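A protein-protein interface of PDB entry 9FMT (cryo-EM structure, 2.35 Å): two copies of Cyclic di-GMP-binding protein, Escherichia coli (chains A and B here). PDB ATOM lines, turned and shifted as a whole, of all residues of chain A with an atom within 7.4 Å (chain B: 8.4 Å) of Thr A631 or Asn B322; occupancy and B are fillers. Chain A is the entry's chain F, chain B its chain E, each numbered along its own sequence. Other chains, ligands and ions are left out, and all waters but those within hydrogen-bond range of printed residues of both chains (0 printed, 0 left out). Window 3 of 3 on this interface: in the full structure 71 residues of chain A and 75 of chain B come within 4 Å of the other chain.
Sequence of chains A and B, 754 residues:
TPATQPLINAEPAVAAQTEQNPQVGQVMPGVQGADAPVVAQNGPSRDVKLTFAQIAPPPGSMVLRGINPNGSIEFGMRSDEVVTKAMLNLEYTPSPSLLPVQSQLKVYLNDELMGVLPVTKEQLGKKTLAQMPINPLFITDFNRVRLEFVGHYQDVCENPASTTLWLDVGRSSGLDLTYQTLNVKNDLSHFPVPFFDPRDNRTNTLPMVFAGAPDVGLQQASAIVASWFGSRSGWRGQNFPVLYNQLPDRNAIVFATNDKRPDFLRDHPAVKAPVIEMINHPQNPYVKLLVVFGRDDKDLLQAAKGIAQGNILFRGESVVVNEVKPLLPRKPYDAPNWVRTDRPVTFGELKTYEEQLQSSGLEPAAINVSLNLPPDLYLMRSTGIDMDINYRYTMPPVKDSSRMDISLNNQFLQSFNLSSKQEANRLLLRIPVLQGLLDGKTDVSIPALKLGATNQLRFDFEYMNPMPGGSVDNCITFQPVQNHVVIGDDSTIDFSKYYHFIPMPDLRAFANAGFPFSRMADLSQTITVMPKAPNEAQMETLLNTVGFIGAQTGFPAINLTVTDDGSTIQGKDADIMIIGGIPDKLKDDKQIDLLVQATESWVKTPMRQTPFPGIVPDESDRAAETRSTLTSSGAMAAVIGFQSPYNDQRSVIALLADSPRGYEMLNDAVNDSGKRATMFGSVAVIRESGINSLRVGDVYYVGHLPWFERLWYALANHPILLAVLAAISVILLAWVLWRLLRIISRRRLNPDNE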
ATOM      1  N   ALA A 598      12.727  24.874  32.193  1.00  0.00           N
ATOM      2  CA  ALA A 598      11.585  24.706  31.302  1.00  0.00           C
ATOM      3  C   ALA A 598      12.013  24.583  29.847  1.00  0.00           C
ATOM      4  O   ALA A 598      11.676  23.595  29.188  1.00  0.00           O
ATOM      5  CB  ALA A 598      10.603  25.871  31.483  1.00  0.00           C
ATOM      6  N   THR A 599      12.749  25.566  29.328  1.00  0.00           N
ATOM      7  CA  THR A 599      13.329  25.510  27.993  1.00  0.00           C
ATOM      8  C   THR A 599      14.773  25.977  27.959  1.00  0.00           C
ATOM      9  O   THR A 599      15.416  25.855  26.910  1.00  0.00           O
ATOM     10  CB  THR A 599      12.517  26.357  26.997  1.00  0.00           C
ATOM     11  OG1 THR A 599      12.693  27.747  27.294  1.00  0.00           O
ATOM     12  CG2 THR A 599      11.035  26.008  27.044  1.00  0.00           C
ATOM     13  N   GLU A 600      15.298  26.510  29.057  1.00  0.00           N
ATOM     14  CA  GLU A 600      16.679  26.958  29.145  1.00  0.00           C
ATOM     15  C   GLU A 600      17.522  25.864  29.782  1.00  0.00           C
ATOM     16  O   GLU A 600      17.175  25.349  30.850  1.00  0.00           O
ATOM     17  CB  GLU A 600      16.773  28.253  29.955  1.00  0.00           C
ATOM     18  CG  GLU A 600      18.187  28.758  30.182  1.00  0.00           C
ATOM     19  CD  GLU A 600      18.746  28.331  31.525  1.00  0.00           C
ATOM     20  OE1 GLU A 600      17.984  28.337  32.515  1.00  0.00           O
ATOM     21  OE2 GLU A 600      19.944  27.987  31.592  1.00  0.00           O
ATOM     22  N   SER A 601      18.628  25.518  29.131  1.00  0.00           N
ATOM     23  CA  SER A 601      19.492  24.442  29.591  1.00  0.00           C
ATOM     24  C   SER A 601      20.947  24.845  29.420  1.00  0.00           C
ATOM     25  O   SER A 601      21.316  25.463  28.418  1.00  0.00           O
ATOM     26  CB  SER A 601      19.220  23.144  28.827  1.00  0.00           C
ATOM     27  OG  SER A 601      19.261  23.359  27.427  1.00  0.00           O
ATOM     28  N   TRP A 602      21.767  24.494  30.405  1.00  0.00           N
ATOM     29  CA  TRP A 602      23.201  24.718  30.345  1.00  0.00           C
ATOM     30  C   TRP A 602      23.925  23.427  30.693  1.00  0.00           C
ATOM     31  O   TRP A 602      23.414  22.595  31.447  1.00  0.00           O
ATOM     32  CB  TRP A 602      23.643  25.847  31.288  1.00  0.00           C
ATOM     33  CG  TRP A 602      23.236  25.654  32.713  1.00  0.00           C
ATOM     34  CD1 TRP A 602      22.124  26.154  33.321  1.00  0.00           C
ATOM     35  CD2 TRP A 602      23.944  24.918  33.716  1.00  0.00           C
ATOM     36  NE1 TRP A 602      22.092  25.769  34.638  1.00  0.00           N
ATOM     37  CE2 TRP A 602      23.199  25.010  34.905  1.00  0.00           C
ATOM     38  CE3 TRP A 602      25.135  24.188  33.722  1.00  0.00           C
ATOM     39  CZ2 TRP A 602      23.605  24.401  36.087  1.00  0.00           C
ATOM     40  CZ3 TRP A 602      25.535  23.584  34.896  1.00  0.00           C
ATOM     41  CH2 TRP A 602      24.772  23.692  36.061  1.00  0.00           C
ATOM     42  N   SER A 628      28.003  26.436  28.523  1.00  0.00           N
ATOM     43  CA  SER A 628      27.195  26.995  27.449  1.00  0.00           C
ATOM     44  C   SER A 628      25.718  26.866  27.796  1.00  0.00           C
ATOM     45  O   SER A 628      25.246  25.773  28.117  1.00  0.00           O
ATOM     46  CB  SER A 628      27.491  26.295  26.121  1.00  0.00           C
ATOM     47  OG  SER A 628      27.617  24.897  26.301  1.00  0.00           O
ATOM     48  N   THR A 629      24.999  27.982  27.727  1.00  0.00           N
ATOM     49  CA  THR A 629      23.570  28.029  28.000  1.00  0.00           C
ATOM     50  C   THR A 629      22.815  28.197  26.690  1.00  0.00           C
ATOM     51  O   THR A 629      23.097  29.125  25.923  1.00  0.00           O
ATOM     52  CB  THR A 629      23.228  29.175  28.954  1.00  0.00           C
ATOM     53  OG1 THR A 629      23.840  28.939  30.228  1.00  0.00           O
ATOM     54  CG2 THR A 629      21.725  29.287  29.133  1.00  0.00           C
ATOM     55  N   LEU A 630      21.865  27.304  26.436  1.00  0.00           N
ATOM     56  CA  LEU A 630      21.092  27.313  25.204  1.00  0.00           C
ATOM     57  C   LEU A 630      19.608  27.247  25.530  1.00  0.00           C
ATOM     58  O   LEU A 630      19.201  26.631  26.518  1.00  0.00           O
ATOM     59  CB  LEU A 630      21.480  26.142  24.291  1.00  0.00           C
ATOM     60  CG  LEU A 630      22.728  26.312  23.421  1.00  0.00           C
ATOM     61  CD1 LEU A 630      23.996  26.081  24.227  1.00  0.00           C
ATOM     62  CD2 LEU A 630      22.677  25.371  22.235  1.00  0.00           C
ATOM     63  N   THR A 631      18.803  27.890  24.689  1.00  0.00           N
ATOM     64  CA  THR A 631      17.357  27.929  24.857  1.00  0.00           C
ATOM     65  C   THR A 631      16.691  27.495  23.561  1.00  0.00           C
ATOM     66  O   THR A 631      16.969  28.060  22.500  1.00  0.00           O
ATOM     67  CB  THR A 631      16.875  29.329  25.254  1.00  0.00           C
ATOM     68  OG1 THR A 631      17.534  29.739  26.459  1.00  0.00           O
ATOM     69  CG2 THR A 631      15.374  29.332  25.481  1.00  0.00           C
ATOM     70  N   SER A 632      15.813  26.499  23.651  1.00  0.00           N
ATOM     71  CA  SER A 632      15.090  26.015  22.486  1.00  0.00           C
ATOM     72  C   SER A 632      13.761  25.426  22.933  1.00  0.00           C
ATOM     73  O   SER A 632      13.585  25.043  24.092  1.00  0.00           O
ATOM     74  CB  SER A 632      15.898  24.972  21.710  1.00  0.00           C
ATOM     75  OG  SER A 632      15.090  24.308  20.754  1.00  0.00           O
ATOM     76  N   SER A 633      12.825  25.355  21.989  1.00  0.00           N
ATOM     77  CA  SER A 633      11.523  24.756  22.235  1.00  0.00           C
ATOM     78  C   SER A 633      11.525  23.245  22.049  1.00  0.00           C
ATOM     79  O   SER A 633      10.507  22.602  22.320  1.00  0.00           O
ATOM     80  CB  SER A 633      10.470  25.383  21.317  1.00  0.00           C
ATOM     81  OG  SER A 633       9.441  24.458  21.013  1.00  0.00           O
ATOM     82  N   GLY A 634      12.635  22.672  21.594  1.00  0.00           N
ATOM     83  CA  GLY A 634      12.730  21.237  21.445  1.00  0.00           C
ATOM     84  C   GLY A 634      12.759  20.528  22.782  1.00  0.00           C
ATOM     85  O   GLY A 634      12.966  21.120  23.842  1.00  0.00           O
ATOM     86  N   LEU B 188      17.497  19.568  15.084  1.00  0.00           N
ATOM     87  CA  LEU B 188      18.868  19.839  15.486  1.00  0.00           C
ATOM     88  C   LEU B 188      19.399  18.833  16.496  1.00  0.00           C
ATOM     89  O   LEU B 188      20.543  18.970  16.938  1.00  0.00           O
ATOM     90  CB  LEU B 188      18.983  21.256  16.055  1.00  0.00           C
ATOM     91  CG  LEU B 188      18.975  22.396  15.036  1.00  0.00           C
ATOM     92  CD1 LEU B 188      18.686  23.718  15.721  1.00  0.00           C
ATOM     93  CD2 LEU B 188      20.295  22.458  14.291  1.00  0.00           C
ATOM     94  N   LYS B 272      17.081  39.197  18.555  1.00  0.00           N
ATOM     95  CA  LYS B 272      17.588  39.839  19.758  1.00  0.00           C
ATOM     96  C   LYS B 272      18.732  39.065  20.393  1.00  0.00           C
ATOM     97  O   LYS B 272      19.291  39.521  21.396  1.00  0.00           O
ATOM     98  CB  LYS B 272      16.460  40.020  20.779  1.00  0.00           C
ATOM     99  CG  LYS B 272      15.163  40.562  20.200  1.00  0.00           C
ATOM    100  CD  LYS B 272      15.383  41.870  19.455  1.00  0.00           C
ATOM    101  CE  LYS B 272      14.106  42.338  18.775  1.00  0.00           C
ATOM    102  NZ  LYS B 272      13.203  41.200  18.446  1.00  0.00           N
ATOM    103  N   ALA B 273      19.092  37.912  19.841  1.00  0.00           N
ATOM    104  CA  ALA B 273      20.148  37.070  20.381  1.00  0.00           C
ATOM    105  C   ALA B 273      20.641  36.158  19.271  1.00  0.00           C
ATOM    106  O   ALA B 273      19.924  35.931  18.289  1.00  0.00           O
ATOM    107  CB  ALA B 273      19.644  36.248  21.579  1.00  0.00           C
ATOM    108  N   PRO B 274      21.860  35.628  19.385  1.00  0.00           N
ATOM    109  CA  PRO B 274      22.350  34.686  18.367  1.00  0.00           C
ATOM    110  C   PRO B 274      21.490  33.434  18.319  1.00  0.00           C
ATOM    111  O   PRO B 274      21.360  32.709  19.308  1.00  0.00           O
ATOM    112  CB  PRO B 274      23.779  34.380  18.827  1.00  0.00           C
ATOM    113  CG  PRO B 274      23.818  34.773  20.265  1.00  0.00           C
ATOM    114  CD  PRO B 274      22.893  35.933  20.387  1.00  0.00           C
ATOM    115  N   VAL B 275      20.901  33.181  17.154  1.00  0.00           N
ATOM    116  CA  VAL B 275      19.981  32.067  16.958  1.00  0.00           C
ATOM    117  C   VAL B 275      20.453  31.248  15.765  1.00  0.00           C
ATOM    118  O   VAL B 275      20.794  31.807  14.716  1.00  0.00           O
ATOM    119  CB  VAL B 275      18.533  32.556  16.756  1.00  0.00           C
ATOM    120  CG1 VAL B 275      18.466  33.626  15.679  1.00  0.00           C
ATOM    121  CG2 VAL B 275      17.614  31.394  16.422  1.00  0.00           C
ATOM    122  N   ILE B 276      20.491  29.929  15.932  1.00  0.00           N
ATOM    123  CA  ILE B 276      20.854  28.996  14.872  1.00  0.00           C
ATOM    124  C   ILE B 276      19.632  28.148  14.553  1.00  0.00           C
ATOM    125  O   ILE B 276      19.032  27.550  15.454  1.00  0.00           O
ATOM    126  CB  ILE B 276      22.045  28.113  15.276  1.00  0.00           C
ATOM    127  CG1 ILE B 276      23.103  28.946  16.000  1.00  0.00           C
ATOM    128  CG2 ILE B 276      22.642  27.434  14.057  1.00  0.00           C
ATOM    129  CD1 ILE B 276      23.909  28.159  16.998  1.00  0.00           C
ATOM    130  N   ARG B 295      22.611  39.659  16.003  1.00  0.00           N
ATOM    131  CA  ARG B 295      22.504  41.109  15.883  1.00  0.00           C
ATOM    132  C   ARG B 295      23.731  41.699  15.204  1.00  0.00           C
ATOM    133  O   ARG B 295      23.615  42.632  14.400  1.00  0.00           O
ATOM    134  CB  ARG B 295      22.309  41.741  17.260  1.00  0.00           C
ATOM    135  CG  ARG B 295      21.056  41.299  17.983  1.00  0.00           C
ATOM    136  CD  ARG B 295      21.012  41.872  19.388  1.00  0.00           C
ATOM    137  NE  ARG B 295      22.051  41.309  20.241  1.00  0.00           N
ATOM    138  CZ  ARG B 295      21.942  41.161  21.554  1.00  0.00           C
ATOM    139  NH1 ARG B 295      20.848  41.525  22.202  1.00  0.00           N
ATOM    140  NH2 ARG B 295      22.956  40.632  22.234  1.00  0.00           N
ATOM    141  N   ASP B 299      27.585  38.697  18.288  1.00  0.00           N
ATOM    142  CA  ASP B 299      26.546  37.677  18.380  1.00  0.00           C
ATOM    143  C   ASP B 299      26.876  36.474  17.505  1.00  0.00           C
ATOM    144  O   ASP B 299      26.667  35.324  17.912  1.00  0.00           O
ATOM    145  CB  ASP B 299      25.194  38.268  17.991  1.00  0.00           C
ATOM    146  CG  ASP B 299      24.452  38.845  19.175  1.00  0.00           C
ATOM    147  OD1 ASP B 299      25.077  39.027  20.239  1.00  0.00           O
ATOM    148  OD2 ASP B 299      23.239  39.114  19.044  1.00  0.00           O
ATOM    149  N   GLN B 302      29.462  34.493  19.270  1.00  0.00           N
ATOM    150  CA  GLN B 302      28.862  33.731  20.360  1.00  0.00           C
ATOM    151  C   GLN B 302      28.143  32.496  19.833  1.00  0.00           C
ATOM    152  O   GLN B 302      28.229  31.416  20.431  1.00  0.00           O
ATOM    153  CB  GLN B 302      27.901  34.618  21.150  1.00  0.00           C
ATOM    154  CG  GLN B 302      27.102  33.882  22.208  1.00  0.00           C
ATOM    155  CD  GLN B 302      27.197  34.537  23.568  1.00  0.00           C
ATOM    156  OE1 GLN B 302      28.291  34.761  24.086  1.00  0.00           O
ATOM    157  NE2 GLN B 302      26.049  34.848  24.157  1.00  0.00           N
ATOM    158  N   ALA B 303      27.434  32.633  18.712  1.00  0.00           N
ATOM    159  CA  ALA B 303      26.763  31.483  18.113  1.00  0.00           C
ATOM    160  C   ALA B 303      27.769  30.439  17.642  1.00  0.00           C
ATOM    161  O   ALA B 303      27.542  29.233  17.793  1.00  0.00           O
ATOM    162  CB  ALA B 303      25.876  31.937  16.957  1.00  0.00           C
ATOM    163  N   GLY B 306      28.979  28.633  20.636  1.00  0.00           N
ATOM    164  CA  GLY B 306      27.952  27.711  21.091  1.00  0.00           C
ATOM    165  C   GLY B 306      27.885  26.456  20.243  1.00  0.00           C
ATOM    166  O   GLY B 306      27.674  25.357  20.761  1.00  0.00           O
ATOM    167  N   LEU B 313      23.385  20.198  23.391  1.00  0.00           N
ATOM    168  CA  LEU B 313      22.091  20.732  23.784  1.00  0.00           C
ATOM    169  C   LEU B 313      21.251  21.175  22.594  1.00  0.00           C
ATOM    170  O   LEU B 313      20.183  21.762  22.786  1.00  0.00           O
ATOM    171  CB  LEU B 313      22.274  21.901  24.754  1.00  0.00           C
ATOM    172  CG  LEU B 313      22.954  21.594  26.088  1.00  0.00           C
ATOM    173  CD1 LEU B 313      22.800  22.765  27.041  1.00  0.00           C
ATOM    174  CD2 LEU B 313      22.391  20.326  26.702  1.00  0.00           C
ATOM    175  N   PHE B 314      21.710  20.914  21.373  1.00  0.00           N
ATOM    176  CA  PHE B 314      20.969  21.316  20.187  1.00  0.00           C
ATOM    177  C   PHE B 314      19.683  20.509  20.074  1.00  0.00           C
ATOM    178  O   PHE B 314      19.698  19.279  20.174  1.00  0.00           O
ATOM    179  CB  PHE B 314      21.823  21.115  18.938  1.00  0.00           C
ATOM    180  CG  PHE B 314      22.693  22.288  18.598  1.00  0.00           C
ATOM    181  CD1 PHE B 314      23.334  23.005  19.592  1.00  0.00           C
ATOM    182  CD2 PHE B 314      22.875  22.668  17.283  1.00  0.00           C
ATOM    183  CE1 PHE B 314      24.136  24.079  19.276  1.00  0.00           C
ATOM    184  CE2 PHE B 314      23.676  23.740  16.964  1.00  0.00           C
ATOM    185  CZ  PHE B 314      24.308  24.447  17.961  1.00  0.00           C
ATOM    186  N   ARG B 315      18.567  21.200  19.862  1.00  0.00           N
ATOM    187  CA  ARG B 315      17.277  20.537  19.751  1.00  0.00           C
ATOM    188  C   ARG B 315      16.316  21.446  19.003  1.00  0.00           C
ATOM    189  O   ARG B 315      16.509  22.662  18.935  1.00  0.00           O
ATOM    190  CB  ARG B 315      16.711  20.181  21.128  1.00  0.00           C
ATOM    191  CG  ARG B 315      16.653  21.353  22.088  1.00  0.00           C
ATOM    192  CD  ARG B 315      16.677  20.891  23.528  1.00  0.00           C
ATOM    193  NE  ARG B 315      16.284  21.953  24.446  1.00  0.00           N
ATOM    194  CZ  ARG B 315      17.115  22.854  24.952  1.00  0.00           C
ATOM    195  NH1 ARG B 315      18.407  22.841  24.669  1.00  0.00           N
ATOM    196  NH2 ARG B 315      16.637  23.793  25.763  1.00  0.00           N
ATOM    197  N   SER B 318      15.055  25.461  15.761  1.00  0.00           N
ATOM    198  CA  SER B 318      15.960  26.567  16.021  1.00  0.00           C
ATOM    199  C   SER B 318      16.387  26.552  17.480  1.00  0.00           C
ATOM    200  O   SER B 318      15.645  26.106  18.357  1.00  0.00           O
ATOM    201  CB  SER B 318      15.312  27.915  15.687  1.00  0.00           C
ATOM    202  OG  SER B 318      14.672  28.465  16.824  1.00  0.00           O
ATOM    203  N   VAL B 319      17.595  27.048  17.729  1.00  0.00           N
ATOM    204  CA  VAL B 319      18.140  27.160  19.074  1.00  0.00           C
ATOM    205  C   VAL B 319      18.714  28.559  19.243  1.00  0.00           C
ATOM    206  O   VAL B 319      19.110  29.210  18.271  1.00  0.00           O
ATOM    207  CB  VAL B 319      19.212  26.081  19.354  1.00  0.00           C
ATOM    208  CG1 VAL B 319      20.556  26.480  18.766  1.00  0.00           C
ATOM    209  CG2 VAL B 319      19.331  25.818  20.844  1.00  0.00           C
ATOM    210  N   VAL B 320      18.739  29.031  20.485  1.00  0.00           N
ATOM    211  CA  VAL B 320      19.247  30.355  20.820  1.00  0.00           C
ATOM    212  C   VAL B 320      20.409  30.183  21.784  1.00  0.00           C
ATOM    213  O   VAL B 320      20.259  29.554  22.839  1.00  0.00           O
ATOM    214  CB  VAL B 320      18.158  31.250  21.431  1.00  0.00           C
ATOM    215  CG1 VAL B 320      18.753  32.571  21.878  1.00  0.00           C
ATOM    216  CG2 VAL B 320      17.037  31.477  20.433  1.00  0.00           C
ATOM    217  N   VAL B 321      21.560  30.739  21.426  1.00  0.00           N
ATOM    218  CA  VAL B 321      22.742  30.697  22.277  1.00  0.00           C
ATOM    219  C   VAL B 321      22.677  31.879  23.234  1.00  0.00           C
ATOM    220  O   VAL B 321      22.659  33.037  22.805  1.00  0.00           O
ATOM    221  CB  VAL B 321      24.032  30.730  21.444  1.00  0.00           C
ATOM    222  CG1 VAL B 321      25.232  30.422  22.320  1.00  0.00           C
ATOM    223  CG2 VAL B 321      23.941  29.748  20.293  1.00  0.00           C
ATOM    224  N   ASN B 322      22.640  31.588  24.531  1.00  0.00           N
ATOM    225  CA  ASN B 322      22.512  32.631  25.540  1.00  0.00           C
ATOM    226  C   ASN B 322      23.867  33.093  26.056  1.00  0.00           C
ATOM    227  O   ASN B 322      24.147  34.296  26.083  1.00  0.00           O
ATOM    228  CB  ASN B 322      21.642  32.136  26.697  1.00  0.00           C
ATOM    229  CG  ASN B 322      20.185  32.005  26.314  1.00  0.00           C
ATOM    230  OD1 ASN B 322      19.392  31.406  27.038  1.00  0.00           O
ATOM    231  ND2 ASN B 322      19.822  32.568  25.169  1.00  0.00           N
ATOM    232  N   GLU B 323      24.719  32.158  26.466  1.00  0.00           N
ATOM    233  CA  GLU B 323      26.031  32.508  26.986  1.00  0.00           C
ATOM    234  C   GLU B 323      26.944  31.296  26.896  1.00  0.00           C
ATOM    235  O   GLU B 323      26.548  30.186  27.258  1.00  0.00           O
ATOM    236  CB  GLU B 323      25.942  32.998  28.435  1.00  0.00           C
ATOM    237  CG  GLU B 323      27.266  33.460  29.019  1.00  0.00           C
ATOM    238  CD  GLU B 323      27.120  34.017  30.421  1.00  0.00           C
ATOM    239  OE1 GLU B 323      25.986  34.021  30.945  1.00  0.00           O
ATOM    240  OE2 GLU B 323      28.138  34.452  30.998  1.00  0.00           O
ATOM    241  N   VAL B 324      28.163  31.518  26.415  1.00  0.00           N
ATOM    242  CA  VAL B 324      29.208  30.501  26.387  1.00  0.00           C
ATOM    243  C   VAL B 324      30.319  31.012  27.292  1.00  0.00           C
ATOM    244  O   VAL B 324      31.119  31.867  26.890  1.00  0.00           O
ATOM    245  CB  VAL B 324      29.716  30.223  24.970  1.00  0.00           C
ATOM    246  CG1 VAL B 324      30.720  29.081  24.982  1.00  0.00           C
ATOM    247  CG2 VAL B 324      28.555  29.904  24.046  1.00  0.00           C
ATOM    248  N   LYS B 325      30.378  30.491  28.515  1.00  0.00           N
ATOM    249  CA  LYS B 325      31.280  31.010  29.530  1.00  0.00           C
ATOM    250  C   LYS B 325      32.455  30.065  29.711  1.00  0.00           C
ATOM    251  O   LYS B 325      32.268  28.955  30.234  1.00  0.00           O
ATOM    252  CB  LYS B 325      30.538  31.198  30.851  1.00  0.00           C
ATOM    253  CG  LYS B 325      31.432  31.481  32.044  1.00  0.00           C
ATOM    254  CD  LYS B 325      30.612  31.612  33.315  1.00  0.00           C
ATOM    255  CE  LYS B 325      31.499  31.586  34.548  1.00  0.00           C
ATOM    256  NZ  LYS B 325      30.811  30.958  35.709  1.00  0.00           N
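The backbone carbonyl oxygen of Thr A599 lies within hydrogen-bond range of the guanidinium group of Arg B315 (2.7 Å). The guanidinium group (NH1) of Arg B315 lies within hydrogen-bond range of the side-chain hydroxyl (OG) of Ser A601, 2.9 Å away. The backbone carbonyl oxygen (O) of Arg B315 lies within hydrogen-bond range of the side-chain hydroxyl (OG) of Ser A632. The guanidinium group (NE) of Arg B315 is in hydrogen-bond range of the backbone carbonyl oxygen (O) of Gly A634 (3.5 Å). O of Ser B318 sits at hydrogen-bond distance from OG of Ser A632 (3.0 Å). O of Thr A631 lies within hydrogen-bond range of N of Val B320, 2.9 Å away. The backbone NH (N) of Asn B322 is in hydrogen-bond range of the backbone carbonyl oxygen (O) of Thr A629 (2.9 Å). The side-chain hydroxyl of Thr A631 is in hydrogen-bond range of the side-chain amide oxygen of Asn B322 (2.6 Å). The backbone carbonyl oxygen (O) of Glu B323 lies within hydrogen-bond range of the backbone NH (N) of Thr A629.
N of Val B321 is in hydrogen-bond range of O of Pro B274 (2.9 Å). The backbone carbonyl oxygen (O) of Ile B276 is in hydrogen-bond range of the backbone NH (N) of Val B319 (2.7 Å). O of Asn B322 lies within hydrogen-bond range of NE2 of Gln B302 (2.8 Å). NH1 of Arg B315 lies within hydrogen-bond range of O of Leu B313, at 2.8 Å. O of Thr A599 is in hydrogen-bond range of N of Ser A632, at 3.3 Å. The side-chain hydroxyl (OG) of Ser A632 sits at hydrogen-bond distance from the backbone NH (N) of Gly A634, at 3.1 Å.
Leu B313 touches Ser A601. Trp A602 touches Leu B313 (CA to CD1, 3.9 Å). Glu B323 touches Ser A628. Val B321 touches Thr A629 (C to O, 3.9 Å). CE1 of Phe B314 touches CD2 of Leu A630, at 3.5 Å. NH2 of Arg B315 touches O of Leu A630 (3.9 Å). Leu A630 touches Val B319 (CD2 to CG2, 3.7 Å). Val B320 touches Leu A630 (O to CA, 3.4 Å). Thr A631 touches Val B319. Ser A632 touches Val B319 (CB to CG2, 3.6 Å).
Printed residues of chain B within 4 Å of Ser A628: Glu B323 (3.3 Å). Thr A631 touches three residues of chain B. Of the printed residues of chain A, Arg B315 touches Thr A599 (2.7 Å), Ser A601 (2.9 Å), Leu A630 (3.9 Å), Ser A632 (2.8 Å) and Gly A634 (3.5 Å). Asn B322 touches just these residues of chain A: Thr A629 and Thr A631. The nearest residue of chain B that does not touch Thr A631 is Arg B315 (4.3 Å). The nearest residue of chain A that does not touch Asn B322 is Glu A600 (4.3 Å). The nearest printed residue of chain B that does not touch Thr A599 is Asn B322 (6.8 Å).
Printed residues of chain B that touch a printed residue of chain A: Leu B313, Phe B314, Arg B315, Ser B318, Val B319, Val B320, Val B321, Asn B322 and Glu B323. Of the 12 printed residues of chain A, 9 touch a printed residue of chain B. Among the printed residues, 19 pairs touch across the chains.
No position is printed for both chains.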
